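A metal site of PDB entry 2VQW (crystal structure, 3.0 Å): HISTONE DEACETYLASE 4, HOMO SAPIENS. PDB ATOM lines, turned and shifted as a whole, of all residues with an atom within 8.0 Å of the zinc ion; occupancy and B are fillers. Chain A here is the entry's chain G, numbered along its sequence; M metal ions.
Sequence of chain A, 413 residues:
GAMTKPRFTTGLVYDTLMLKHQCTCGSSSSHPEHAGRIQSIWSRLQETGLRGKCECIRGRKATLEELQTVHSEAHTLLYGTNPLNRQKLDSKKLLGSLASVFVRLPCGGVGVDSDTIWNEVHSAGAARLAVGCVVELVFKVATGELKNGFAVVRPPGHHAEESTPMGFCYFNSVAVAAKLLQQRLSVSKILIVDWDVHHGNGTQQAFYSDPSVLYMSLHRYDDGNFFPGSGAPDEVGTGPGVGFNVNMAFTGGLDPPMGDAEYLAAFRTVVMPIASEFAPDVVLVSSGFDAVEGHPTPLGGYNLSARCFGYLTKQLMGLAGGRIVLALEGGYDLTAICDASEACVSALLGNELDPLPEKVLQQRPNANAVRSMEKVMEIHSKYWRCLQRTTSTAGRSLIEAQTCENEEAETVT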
ATOM      1  N   GLN A  22       1.055   1.144  27.703  1.00  0.00           N
ATOM      2  CA  GLN A  22       1.030   2.483  28.267  1.00  0.00           C
ATOM      3  C   GLN A  22       2.355   3.168  27.996  1.00  0.00           C
ATOM      4  O   GLN A  22       3.368   2.500  27.788  1.00  0.00           O
ATOM      5  CB  GLN A  22       0.771   2.433  29.769  1.00  0.00           C
ATOM      6  CG  GLN A  22      -0.674   2.196  30.168  1.00  0.00           C
ATOM      7  CD  GLN A  22      -0.854   2.055  31.672  1.00  0.00           C
ATOM      8  OE1 GLN A  22      -0.382   2.898  32.442  1.00  0.00           O
ATOM      9  NE2 GLN A  22      -1.544   0.999  32.095  1.00  0.00           N
ATOM     10  N   CYS A  23       2.339   4.500  27.980  1.00  0.00           N
ATOM     11  CA  CYS A  23       3.571   5.266  27.755  1.00  0.00           C
ATOM     12  C   CYS A  23       4.564   5.043  28.880  1.00  0.00           C
ATOM     13  O   CYS A  23       4.172   4.891  30.046  1.00  0.00           O
ATOM     14  CB  CYS A  23       3.278   6.764  27.630  1.00  0.00           C
ATOM     15  SG  CYS A  23       4.733   7.716  27.174  1.00  0.00           S
ATOM     16  N   THR A  24       5.846   5.038  28.524  1.00  0.00           N
ATOM     17  CA  THR A  24       6.928   4.756  29.471  1.00  0.00           C
ATOM     18  C   THR A  24       7.003   5.765  30.628  1.00  0.00           C
ATOM     19  O   THR A  24       7.619   5.489  31.649  1.00  0.00           O
ATOM     20  CB  THR A  24       8.300   4.652  28.768  1.00  0.00           C
ATOM     21  OG1 THR A  24       8.535   5.848  28.010  1.00  0.00           O
ATOM     22  CG2 THR A  24       8.342   3.434  27.845  1.00  0.00           C
ATOM     23  N   CYS A  25       6.367   6.924  30.450  1.00  0.00           N
ATOM     24  CA  CYS A  25       6.162   7.857  31.557  1.00  0.00           C
ATOM     25  C   CYS A  25       4.897   7.454  32.312  1.00  0.00           C
ATOM     26  O   CYS A  25       4.431   8.170  33.199  1.00  0.00           O
ATOM     27  CB  CYS A  25       6.077   9.303  31.059  1.00  0.00           C
ATOM     28  SG  CYS A  25       4.570   9.739  30.137  1.00  0.00           S
ATOM     29  N   SER A  29      -2.478  10.335  30.825  1.00  0.00           N
ATOM     30  CA  SER A  29      -1.691  11.504  31.216  1.00  0.00           C
ATOM     31  C   SER A  29      -1.937  12.670  30.251  1.00  0.00           C
ATOM     32  O   SER A  29      -2.897  13.423  30.401  1.00  0.00           O
ATOM     33  CB  SER A  29      -0.196  11.137  31.277  1.00  0.00           C
ATOM     34  OG  SER A  29       0.023   9.945  32.021  1.00  0.00           O
ATOM     35  N   SER A  30      -1.056  12.831  29.262  1.00  0.00           N
ATOM     36  CA  SER A  30      -1.278  13.734  28.137  1.00  0.00           C
ATOM     37  C   SER A  30      -1.609  12.918  26.882  1.00  0.00           C
ATOM     38  O   SER A  30      -1.395  13.354  25.750  1.00  0.00           O
ATOM     39  CB  SER A  30      -0.042  14.610  27.893  1.00  0.00           C
ATOM     40  OG  SER A  30       1.080  13.809  27.569  1.00  0.00           O
ATOM     41  N   HIS A  31      -2.140  11.712  27.119  1.00  0.00           N
ATOM     42  CA  HIS A  31      -2.465  10.753  26.074  1.00  0.00           C
ATOM     43  C   HIS A  31      -3.937  10.371  26.151  1.00  0.00           C
ATOM     44  O   HIS A  31      -4.336   9.687  27.096  1.00  0.00           O
ATOM     45  CB  HIS A  31      -1.607   9.497  26.219  1.00  0.00           C
ATOM     46  CG  HIS A  31      -0.144   9.779  26.311  1.00  0.00           C
ATOM     47  ND1 HIS A  31       0.652   9.951  25.199  1.00  0.00           N
ATOM     48  CD2 HIS A  31       0.683   9.910  27.381  1.00  0.00           C
ATOM     49  CE1 HIS A  31       1.898  10.186  25.583  1.00  0.00           C
ATOM     50  NE2 HIS A  31       1.941  10.170  26.905  1.00  0.00           N
ATOM     51  N   LEU A 105       9.111  11.693  22.687  1.00  0.00           N
ATOM     52  CA  LEU A 105       7.907  12.506  22.828  1.00  0.00           C
ATOM     53  C   LEU A 105       8.148  13.780  23.652  1.00  0.00           C
ATOM     54  O   LEU A 105       9.178  13.899  24.308  1.00  0.00           O
ATOM     55  CB  LEU A 105       6.773  11.664  23.446  1.00  0.00           C
ATOM     56  CG  LEU A 105       5.754  10.992  22.498  1.00  0.00           C
ATOM     57  CD1 LEU A 105       6.424  10.162  21.418  1.00  0.00           C
ATOM     58  CD2 LEU A 105       4.764  10.141  23.281  1.00  0.00           C
ATOM     59  N   PRO A 106       7.199  14.734  23.602  1.00  0.00           N
ATOM     60  CA  PRO A 106       7.319  15.932  24.441  1.00  0.00           C
ATOM     61  C   PRO A 106       7.020  15.635  25.921  1.00  0.00           C
ATOM     62  O   PRO A 106       7.123  16.533  26.758  1.00  0.00           O
ATOM     63  CB  PRO A 106       6.266  16.873  23.867  1.00  0.00           C
ATOM     64  CG  PRO A 106       5.225  15.969  23.298  1.00  0.00           C
ATOM     65  CD  PRO A 106       5.973  14.782  22.779  1.00  0.00           C
ATOM     66  N   CYS A 107       6.663  14.387  26.224  1.00  0.00           N
ATOM     67  CA  CYS A 107       6.392  13.966  27.594  1.00  0.00           C
ATOM     68  C   CYS A 107       7.538  13.125  28.171  1.00  0.00           C
ATOM     69  O   CYS A 107       7.510  12.736  29.339  1.00  0.00           O
ATOM     70  CB  CYS A 107       5.064  13.193  27.655  1.00  0.00           C
ATOM     71  SG  CYS A 107       5.099  11.553  26.870  1.00  0.00           S
ATOM     72  N   GLY A 108       8.529  12.837  27.334  1.00  0.00           N
ATOM     73  CA  GLY A 108       9.686  12.035  27.752  1.00  0.00           C
ATOM     74  C   GLY A 108       9.644  10.593  27.275  1.00  0.00           C
ATOM     75  O   GLY A 108      10.671   9.922  27.248  1.00  0.00           O
ATOM     76  N   GLY A 109       8.458  10.118  26.902  1.00  0.00           N
ATOM     77  CA  GLY A 109       8.281   8.733  26.480  1.00  0.00           C
ATOM     78  C   GLY A 109       8.733   8.416  25.064  1.00  0.00           C
ATOM     79  O   GLY A 109       9.112   9.302  24.300  1.00  0.00           O
ATOM     80  N   VAL A 110       8.686   7.124  24.718  1.00  0.00           N
ATOM     81  CA  VAL A 110       9.027   6.659  23.387  1.00  0.00           C
ATOM     82  C   VAL A 110       7.767   6.590  22.532  1.00  0.00           C
ATOM     83  O   VAL A 110       6.713   6.193  23.015  1.00  0.00           O
ATOM     84  CB  VAL A 110       9.700   5.276  23.426  1.00  0.00           C
ATOM     85  CG1 VAL A 110      10.159   4.847  22.029  1.00  0.00           C
ATOM     86  CG2 VAL A 110      10.886   5.262  24.387  1.00  0.00           C
ATOM     87  N   ILE A 117       2.112   6.507  21.025  1.00  0.00           N
ATOM     88  CA  ILE A 117       3.166   5.987  21.900  1.00  0.00           C
ATOM     89  C   ILE A 117       3.747   4.679  21.395  1.00  0.00           C
ATOM     90  O   ILE A 117       3.267   4.112  20.416  1.00  0.00           O
ATOM     91  CB  ILE A 117       2.654   5.747  23.332  1.00  0.00           C
ATOM     92  CG1 ILE A 117       1.589   4.649  23.341  1.00  0.00           C
ATOM     93  CG2 ILE A 117       2.138   7.045  23.949  1.00  0.00           C
ATOM     94  CD1 ILE A 117       1.564   3.816  24.598  1.00  0.00           C
HETATM   95 ZN    ZN M   1       3.831   9.798  27.770  1.00  0.00          ZN
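N of Gly 109 sits close to SG of Cys 107, at 3.7 Å.
The zinc ion is bound by NE2 of His 31 (2.1 Å), SG of Cys 107 (2.3 Å), SG of Cys 23 (2.3 Å) and SG of Cys 25 (2.5 Å). The zinc ion has four donor atoms within binding distance.
Four residues have an atom within 4 Å of the zinc ion: Cys 23, Cys 25, His 31 and Cys 107.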
